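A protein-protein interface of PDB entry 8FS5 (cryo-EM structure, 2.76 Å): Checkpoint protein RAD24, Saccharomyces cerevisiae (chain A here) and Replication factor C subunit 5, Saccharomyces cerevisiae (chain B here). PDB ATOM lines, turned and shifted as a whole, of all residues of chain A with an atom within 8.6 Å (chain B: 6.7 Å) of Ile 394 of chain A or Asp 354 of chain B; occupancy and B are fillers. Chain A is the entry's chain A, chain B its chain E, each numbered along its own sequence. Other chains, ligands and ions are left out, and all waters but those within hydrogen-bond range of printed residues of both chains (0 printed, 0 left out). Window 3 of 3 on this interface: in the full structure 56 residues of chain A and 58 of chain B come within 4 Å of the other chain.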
ATOM      1  N   TYR A 384     -34.527  12.778   5.759  1.00  0.00           N
ATOM      2  CA  TYR A 384     -33.961  13.076   4.447  1.00  0.00           C
ATOM      3  C   TYR A 384     -33.923  11.854   3.536  1.00  0.00           C
ATOM      4  O   TYR A 384     -33.684  12.002   2.334  1.00  0.00           O
ATOM      5  CB  TYR A 384     -32.557  13.668   4.594  1.00  0.00           C
ATOM      6  CG  TYR A 384     -31.466  12.645   4.812  1.00  0.00           C
ATOM      7  CD1 TYR A 384     -31.223  12.124   6.072  1.00  0.00           C
ATOM      8  CD2 TYR A 384     -30.668  12.212   3.759  1.00  0.00           C
ATOM      9  CE1 TYR A 384     -30.227  11.191   6.280  1.00  0.00           C
ATOM     10  CE2 TYR A 384     -29.670  11.280   3.958  1.00  0.00           C
ATOM     11  CZ  TYR A 384     -29.455  10.774   5.221  1.00  0.00           C
ATOM     12  OH  TYR A 384     -28.461   9.846   5.427  1.00  0.00           O
ATOM     13  N   GLY A 390     -35.754   6.543  -0.443  1.00  0.00           N
ATOM     14  CA  GLY A 390     -34.406   6.067  -0.247  1.00  0.00           C
ATOM     15  C   GLY A 390     -33.666   5.658  -1.501  1.00  0.00           C
ATOM     16  O   GLY A 390     -32.794   4.786  -1.425  1.00  0.00           O
ATOM     17  N   GLU A 391     -33.980   6.256  -2.652  1.00  0.00           N
ATOM     18  CA  GLU A 391     -33.366   5.847  -3.909  1.00  0.00           C
ATOM     19  C   GLU A 391     -32.612   6.985  -4.586  1.00  0.00           C
ATOM     20  O   GLU A 391     -32.748   7.189  -5.797  1.00  0.00           O
ATOM     21  CB  GLU A 391     -34.426   5.290  -4.864  1.00  0.00           C
ATOM     22  CG  GLU A 391     -35.345   4.250  -4.244  1.00  0.00           C
ATOM     23  CD  GLU A 391     -34.643   2.932  -3.988  1.00  0.00           C
ATOM     24  OE1 GLU A 391     -33.723   2.588  -4.760  1.00  0.00           O
ATOM     25  OE2 GLU A 391     -35.011   2.239  -3.017  1.00  0.00           O
ATOM     26  N   PHE A 392     -31.819   7.732  -3.826  1.00  0.00           N
ATOM     27  CA  PHE A 392     -30.939   8.750  -4.387  1.00  0.00           C
ATOM     28  C   PHE A 392     -29.485   8.336  -4.175  1.00  0.00           C
ATOM     29  O   PHE A 392     -29.190   7.305  -3.563  1.00  0.00           O
ATOM     30  CB  PHE A 392     -31.220  10.131  -3.782  1.00  0.00           C
ATOM     31  CG  PHE A 392     -31.375  10.133  -2.287  1.00  0.00           C
ATOM     32  CD1 PHE A 392     -32.615   9.932  -1.702  1.00  0.00           C
ATOM     33  CD2 PHE A 392     -30.281  10.354  -1.466  1.00  0.00           C
ATOM     34  CE1 PHE A 392     -32.760   9.941  -0.329  1.00  0.00           C
ATOM     35  CE2 PHE A 392     -30.420  10.365  -0.091  1.00  0.00           C
ATOM     36  CZ  PHE A 392     -31.661  10.158   0.477  1.00  0.00           C
ATOM     37  N   SER A 393     -28.574   9.151  -4.700  1.00  0.00           N
ATOM     38  CA  SER A 393     -27.156   8.828  -4.661  1.00  0.00           C
ATOM     39  C   SER A 393     -26.616   8.892  -3.233  1.00  0.00           C
ATOM     40  O   SER A 393     -27.063   9.686  -2.401  1.00  0.00           O
ATOM     41  CB  SER A 393     -26.365   9.779  -5.560  1.00  0.00           C
ATOM     42  OG  SER A 393     -25.021   9.355  -5.693  1.00  0.00           O
ATOM     43  N   ILE A 394     -25.637   8.027  -2.957  1.00  0.00           N
ATOM     44  CA  ILE A 394     -25.003   8.005  -1.644  1.00  0.00           C
ATOM     45  C   ILE A 394     -24.149   9.246  -1.402  1.00  0.00           C
ATOM     46  O   ILE A 394     -23.962   9.644  -0.245  1.00  0.00           O
ATOM     47  CB  ILE A 394     -24.176   6.715  -1.479  1.00  0.00           C
ATOM     48  CG1 ILE A 394     -23.687   6.553  -0.036  1.00  0.00           C
ATOM     49  CG2 ILE A 394     -23.009   6.684  -2.458  1.00  0.00           C
ATOM     50  CD1 ILE A 394     -24.798   6.348   0.967  1.00  0.00           C
ATOM     51  N   SER A 395     -23.638   9.877  -2.462  1.00  0.00           N
ATOM     52  CA  SER A 395     -22.843  11.090  -2.293  1.00  0.00           C
ATOM     53  C   SER A 395     -23.681  12.225  -1.717  1.00  0.00           C
ATOM     54  O   SER A 395     -23.212  12.977  -0.855  1.00  0.00           O
ATOM     55  CB  SER A 395     -22.226  11.502  -3.629  1.00  0.00           C
ATOM     56  OG  SER A 395     -21.750  10.374  -4.341  1.00  0.00           O
ATOM     57  N   ASP A 396     -24.924  12.363  -2.181  1.00  0.00           N
ATOM     58  CA  ASP A 396     -25.806  13.405  -1.665  1.00  0.00           C
ATOM     59  C   ASP A 396     -26.121  13.180  -0.191  1.00  0.00           C
ATOM     60  O   ASP A 396     -26.101  14.124   0.612  1.00  0.00           O
ATOM     61  CB  ASP A 396     -27.091  13.451  -2.492  1.00  0.00           C
ATOM     62  CG  ASP A 396     -26.832  13.755  -3.954  1.00  0.00           C
ATOM     63  OD1 ASP A 396     -26.215  14.802  -4.244  1.00  0.00           O
ATOM     64  OD2 ASP A 396     -27.244  12.948  -4.814  1.00  0.00           O
ATOM     65  N   ALA A 397     -26.413  11.932   0.186  1.00  0.00           N
ATOM     66  CA  ALA A 397     -26.680  11.618   1.585  1.00  0.00           C
ATOM     67  C   ALA A 397     -25.453  11.874   2.450  1.00  0.00           C
ATOM     68  O   ALA A 397     -25.566  12.407   3.561  1.00  0.00           O
ATOM     69  CB  ALA A 397     -27.139  10.168   1.717  1.00  0.00           C
ATOM     70  N   SER A 398     -24.272  11.497   1.955  1.00  0.00           N
ATOM     71  CA  SER A 398     -23.041  11.759   2.691  1.00  0.00           C
ATOM     72  C   SER A 398     -22.808  13.250   2.874  1.00  0.00           C
ATOM     73  O   SER A 398     -22.408  13.681   3.959  1.00  0.00           O
ATOM     74  CB  SER A 398     -21.852  11.119   1.974  1.00  0.00           C
ATOM     75  OG  SER A 398     -21.515  11.842   0.803  1.00  0.00           O
ATOM     76  N   SER A 399     -23.065  14.048   1.833  1.00  0.00           N
ATOM     77  CA  SER A 399     -22.928  15.496   1.956  1.00  0.00           C
ATOM     78  C   SER A 399     -23.900  16.059   2.986  1.00  0.00           C
ATOM     79  O   SER A 399     -23.521  16.908   3.802  1.00  0.00           O
ATOM     80  CB  SER A 399     -23.144  16.160   0.595  1.00  0.00           C
ATOM     81  OG  SER A 399     -22.192  15.708  -0.351  1.00  0.00           O
ATOM     82  N   ILE A 400     -25.150  15.588   2.973  1.00  0.00           N
ATOM     83  CA  ILE A 400     -26.143  16.083   3.924  1.00  0.00           C
ATOM     84  C   ILE A 400     -25.733  15.756   5.357  1.00  0.00           C
ATOM     85  O   ILE A 400     -25.754  16.628   6.237  1.00  0.00           O
ATOM     86  CB  ILE A 400     -27.535  15.512   3.595  1.00  0.00           C
ATOM     87  CG1 ILE A 400     -28.061  16.089   2.282  1.00  0.00           C
ATOM     88  CG2 ILE A 400     -28.512  15.790   4.729  1.00  0.00           C
ATOM     89  CD1 ILE A 400     -29.403  15.527   1.872  1.00  0.00           C
ATOM     90  N   VAL A 401     -25.352  14.504   5.615  1.00  0.00           N
ATOM     91  CA  VAL A 401     -25.012  14.124   6.983  1.00  0.00           C
ATOM     92  C   VAL A 401     -23.704  14.773   7.433  1.00  0.00           C
ATOM     93  O   VAL A 401     -23.567  15.141   8.605  1.00  0.00           O
ATOM     94  CB  VAL A 401     -24.971  12.594   7.134  1.00  0.00           C
ATOM     95  CG1 VAL A 401     -24.833  12.221   8.595  1.00  0.00           C
ATOM     96  CG2 VAL A 401     -26.239  11.979   6.582  1.00  0.00           C
ATOM     97  N   THR A 427     -28.937  20.361  -1.916  1.00  0.00           N
ATOM     98  CA  THR A 427     -28.710  18.976  -2.307  1.00  0.00           C
ATOM     99  C   THR A 427     -29.968  18.356  -2.902  1.00  0.00           C
ATOM    100  O   THR A 427     -29.907  17.675  -3.932  1.00  0.00           O
ATOM    101  CB  THR A 427     -28.226  18.169  -1.099  1.00  0.00           C
ATOM    102  OG1 THR A 427     -26.893  18.569  -0.758  1.00  0.00           O
ATOM    103  CG2 THR A 427     -28.235  16.684  -1.408  1.00  0.00           C
ATOM    104  N   ILE A 431     -30.960  17.117  -7.420  1.00  0.00           N
ATOM    105  CA  ILE A 431     -31.324  15.734  -7.709  1.00  0.00           C
ATOM    106  C   ILE A 431     -32.827  15.585  -7.916  1.00  0.00           C
ATOM    107  O   ILE A 431     -33.300  14.503  -8.287  1.00  0.00           O
ATOM    108  CB  ILE A 431     -30.812  14.808  -6.593  1.00  0.00           C
ATOM    109  CG1 ILE A 431     -31.809  14.761  -5.433  1.00  0.00           C
ATOM    110  CG2 ILE A 431     -29.439  15.257  -6.114  1.00  0.00           C
ATOM    111  CD1 ILE A 431     -31.433  13.785  -4.343  1.00  0.00           C
ATOM    112  N   ARG B 274     -23.869  -0.682   0.104  1.00  0.00           N
ATOM    113  CA  ARG B 274     -23.507   0.735   0.158  1.00  0.00           C
ATOM    114  C   ARG B 274     -24.609   1.526  -0.541  1.00  0.00           C
ATOM    115  O   ARG B 274     -24.531   1.803  -1.740  1.00  0.00           O
ATOM    116  CB  ARG B 274     -22.135   0.976  -0.486  1.00  0.00           C
ATOM    117  CG  ARG B 274     -20.986   0.275   0.219  1.00  0.00           C
ATOM    118  CD  ARG B 274     -19.715   0.319  -0.612  1.00  0.00           C
ATOM    119  NE  ARG B 274     -19.907  -0.262  -1.935  1.00  0.00           N
ATOM    120  CZ  ARG B 274     -19.814  -1.557  -2.204  1.00  0.00           C
ATOM    121  NH1 ARG B 274     -19.535  -2.442  -1.262  1.00  0.00           N
ATOM    122  NH2 ARG B 274     -20.006  -1.976  -3.452  1.00  0.00           N
ATOM    123  N   SER B 275     -25.639   1.892   0.219  1.00  0.00           N
ATOM    124  CA  SER B 275     -26.772   2.632  -0.318  1.00  0.00           C
ATOM    125  C   SER B 275     -27.432   3.408   0.815  1.00  0.00           C
ATOM    126  O   SER B 275     -27.053   3.285   1.984  1.00  0.00           O
ATOM    127  CB  SER B 275     -27.767   1.695  -1.009  1.00  0.00           C
ATOM    128  OG  SER B 275     -28.284   0.739  -0.100  1.00  0.00           O
ATOM    129  N   VAL B 276     -28.428   4.223   0.455  1.00  0.00           N
ATOM    130  CA  VAL B 276     -29.150   5.029   1.439  1.00  0.00           C
ATOM    131  C   VAL B 276     -29.939   4.192   2.432  1.00  0.00           C
ATOM    132  O   VAL B 276     -29.887   4.472   3.636  1.00  0.00           O
ATOM    133  CB  VAL B 276     -30.095   6.020   0.734  1.00  0.00           C
ATOM    134  CG1 VAL B 276     -30.809   6.898   1.751  1.00  0.00           C
ATOM    135  CG2 VAL B 276     -29.320   6.871  -0.259  1.00  0.00           C
ATOM    136  N   LEU B 279     -27.704   2.738   4.802  1.00  0.00           N
ATOM    137  CA  LEU B 279     -27.324   3.773   5.759  1.00  0.00           C
ATOM    138  C   LEU B 279     -28.385   3.956   6.837  1.00  0.00           C
ATOM    139  O   LEU B 279     -28.050   4.158   8.009  1.00  0.00           O
ATOM    140  CB  LEU B 279     -27.067   5.091   5.029  1.00  0.00           C
ATOM    141  CG  LEU B 279     -26.541   6.262   5.856  1.00  0.00           C
ATOM    142  CD1 LEU B 279     -25.249   5.884   6.553  1.00  0.00           C
ATOM    143  CD2 LEU B 279     -26.326   7.472   4.967  1.00  0.00           C
ATOM    144  N   ASN B 317      -8.533   2.639   0.205  1.00  0.00           N
ATOM    145  CA  ASN B 317      -9.771   2.665   0.975  1.00  0.00           C
ATOM    146  C   ASN B 317      -9.508   2.788   2.470  1.00  0.00           C
ATOM    147  O   ASN B 317     -10.174   3.576   3.148  1.00  0.00           O
ATOM    148  CB  ASN B 317     -10.591   1.406   0.691  1.00  0.00           C
ATOM    149  CG  ASN B 317     -11.234   1.425  -0.681  1.00  0.00           C
ATOM    150  OD1 ASN B 317     -11.241   2.451  -1.361  1.00  0.00           O
ATOM    151  ND2 ASN B 317     -11.779   0.288  -1.094  1.00  0.00           N
ATOM    152  N   ILE B 346     -20.041   6.782   8.662  1.00  0.00           N
ATOM    153  CA  ILE B 346     -20.503   5.622   7.903  1.00  0.00           C
ATOM    154  C   ILE B 346     -20.855   6.019   6.476  1.00  0.00           C
ATOM    155  O   ILE B 346     -20.524   5.310   5.517  1.00  0.00           O
ATOM    156  CB  ILE B 346     -21.694   4.957   8.621  1.00  0.00           C
ATOM    157  CG1 ILE B 346     -21.229   4.307   9.926  1.00  0.00           C
ATOM    158  CG2 ILE B 346     -22.365   3.932   7.719  1.00  0.00           C
ATOM    159  CD1 ILE B 346     -22.269   3.425  10.578  1.00  0.00           C
ATOM    160  N   ALA B 347     -21.536   7.158   6.311  1.00  0.00           N
ATOM    161  CA  ALA B 347     -21.894   7.626   4.978  1.00  0.00           C
ATOM    162  C   ALA B 347     -20.666   7.909   4.124  1.00  0.00           C
ATOM    163  O   ALA B 347     -20.630   7.510   2.955  1.00  0.00           O
ATOM    164  CB  ALA B 347     -22.767   8.878   5.077  1.00  0.00           C
ATOM    165  N   LYS B 348     -19.649   8.564   4.689  1.00  0.00           N
ATOM    166  CA  LYS B 348     -18.415   8.799   3.948  1.00  0.00           C
ATOM    167  C   LYS B 348     -17.674   7.502   3.646  1.00  0.00           C
ATOM    168  O   LYS B 348     -17.092   7.366   2.563  1.00  0.00           O
ATOM    169  CB  LYS B 348     -17.512   9.759   4.722  1.00  0.00           C
ATOM    170  CG  LYS B 348     -17.863  11.223   4.521  1.00  0.00           C
ATOM    171  CD  LYS B 348     -16.621  12.097   4.493  1.00  0.00           C
ATOM    172  CE  LYS B 348     -16.975  13.542   4.185  1.00  0.00           C
ATOM    173  NZ  LYS B 348     -17.856  13.654   2.990  1.00  0.00           N
ATOM    174  N   VAL B 349     -17.693   6.542   4.573  1.00  0.00           N
ATOM    175  CA  VAL B 349     -17.047   5.258   4.323  1.00  0.00           C
ATOM    176  C   VAL B 349     -17.706   4.536   3.154  1.00  0.00           C
ATOM    177  O   VAL B 349     -17.021   4.033   2.259  1.00  0.00           O
ATOM    178  CB  VAL B 349     -17.055   4.404   5.605  1.00  0.00           C
ATOM    179  CG1 VAL B 349     -16.873   2.930   5.273  1.00  0.00           C
ATOM    180  CG2 VAL B 349     -15.964   4.870   6.554  1.00  0.00           C
ATOM    181  N   MET B 350     -19.042   4.485   3.126  1.00  0.00           N
ATOM    182  CA  MET B 350     -19.711   3.827   2.005  1.00  0.00           C
ATOM    183  C   MET B 350     -19.580   4.627   0.714  1.00  0.00           C
ATOM    184  O   MET B 350     -19.572   4.042  -0.375  1.00  0.00           O
ATOM    185  CB  MET B 350     -21.184   3.564   2.321  1.00  0.00           C
ATOM    186  CG  MET B 350     -21.437   2.968   3.692  1.00  0.00           C
ATOM    187  SD  MET B 350     -23.093   2.277   3.840  1.00  0.00           S
ATOM    188  CE  MET B 350     -24.083   3.733   3.533  1.00  0.00           C
ATOM    189  N   CYS B 351     -19.479   5.953   0.805  1.00  0.00           N
ATOM    190  CA  CYS B 351     -19.247   6.772  -0.377  1.00  0.00           C
ATOM    191  C   CYS B 351     -17.827   6.639  -0.913  1.00  0.00           C
ATOM    192  O   CYS B 351     -17.590   6.959  -2.083  1.00  0.00           O
ATOM    193  CB  CYS B 351     -19.551   8.241  -0.062  1.00  0.00           C
ATOM    194  SG  CYS B 351     -19.554   9.350  -1.492  1.00  0.00           S
ATOM    195  N   CYS B 352     -16.882   6.188  -0.091  1.00  0.00           N
ATOM    196  CA  CYS B 352     -15.517   5.936  -0.537  1.00  0.00           C
ATOM    197  C   CYS B 352     -15.305   4.508  -1.018  1.00  0.00           C
ATOM    198  O   CYS B 352     -14.538   4.281  -1.958  1.00  0.00           O
ATOM    199  CB  CYS B 352     -14.524   6.258   0.591  1.00  0.00           C
ATOM    200  SG  CYS B 352     -13.992   4.827   1.560  1.00  0.00           S
ATOM    201  N   LEU B 353     -15.966   3.528  -0.394  1.00  0.00           N
ATOM    202  CA  LEU B 353     -15.769   2.133  -0.778  1.00  0.00           C
ATOM    203  C   LEU B 353     -16.472   1.769  -2.080  1.00  0.00           C
ATOM    204  O   LEU B 353     -16.086   0.784  -2.718  1.00  0.00           O
ATOM    205  CB  LEU B 353     -16.251   1.196   0.333  1.00  0.00           C
ATOM    206  CG  LEU B 353     -15.569   1.265   1.699  1.00  0.00           C
ATOM    207  CD1 LEU B 353     -16.216   0.285   2.665  1.00  0.00           C
ATOM    208  CD2 LEU B 353     -14.084   0.990   1.573  1.00  0.00           C
ATOM    209  N   ASP B 354     -17.486   2.526  -2.487  1.00  0.00           N
ATOM    210  CA  ASP B 354     -18.262   2.172  -3.673  1.00  0.00           C
ATOM    211  C   ASP B 354     -17.478   2.401  -4.964  1.00  0.00           C
ATOM    212  O   ASP B 354     -17.878   1.947  -6.036  1.00  0.00           O
ATOM    213  CB  ASP B 354     -19.583   2.953  -3.702  1.00  0.00           C
ATOM    214  CG  ASP B 354     -19.404   4.412  -4.095  1.00  0.00           C
ATOM    215  OD1 ASP B 354     -18.310   4.973  -3.874  1.00  0.00           O
ATOM    216  OD2 ASP B 354     -20.375   5.008  -4.605  1.00  0.00           O
ATOM    217  OXT ASP B 354     -16.428   3.044  -4.964  1.00  0.00           O
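SG of Cys 351 of chain B lies within hydrogen-bond range of OG of Ser 395 of chain A (3.7 Å).
The backbone carbonyl oxygen (O) of Ile 394 of chain A lies close to the side-chain hydroxyl (OG) of Ser 398 of chain A. O of Ser 395 of chain A sits at hydrogen-bond distance from OG of Ser 398 of chain A. The backbone carbonyl oxygen (O) of Ser 395 of chain A sits at hydrogen-bond distance from the side-chain hydroxyl (OG) of Ser 399 of chain A, at 3.0 Å.
Among the printed residues, merely in contact across the chains: Tyr 384 of chain A with Leu 279 of chain B (3.2 Å), Gly 390 of chain A with Val 276 of chain B (3.7 Å), Phe 392 of chain A with Val 276 of chain B (3.3 Å), Ile 394 of chain A with Ser 275 of chain B (3.9 Å), Ile 394 of chain A with Met 350 of chain B (3.7 Å), Ile 394 of chain A with Asp 354 of chain B (3.8 Å), Ser 398 of chain A with Ala 347 of chain B (3.8 Å) and Ser 398 of chain A with Cys 351 of chain B (3.9 Å).
Ile 394 of chain A touches three residues of chain B. Asp 354 of chain B touches just one residue of chain A: Ile 394. Of the printed residues of chain B, Phe 392 of chain A touches Val 276 (3.3 Å). Printed residues of chain A within 4 Å of Met 350 of chain B: Ile 394 (3.7 Å). Printed residues of chain B within 4 Å of Ser 395 of chain A: Cys 351. Asn 317 of chain B touches none of the printed residues of chain A. Ile 400 of chain A touches none of the printed residues of chain B. The nearest residue of chain B that does not touch Ile 394 of chain A is Val 276 of chain B (4.2 Å). The nearest printed residue of chain A that does not touch Met 350 of chain B is Ser 398 of chain A (7.0 Å).
Of the 14 printed residues of chain B, 7 touch a printed residue of chain A. Hydrophobic or aromatic side chains of chain B that line the printed part of chain A: Val 276, Leu 279, Ala 347 and Met 350. Of the 15 printed residues of chain A, 6 touch a printed residue of chain B. Printed residues of chain A that touch a printed residue of chain B: Tyr 384, Gly 390, Phe 392, Ile 394, Ser 395 and Ser 398. Among the printed residues, 9 pairs touch across the chains. Among the printed residues, no Asp or Glu carboxylate lies within 4 Å of a Lys or Arg side-chain nitrogen of the other chain.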
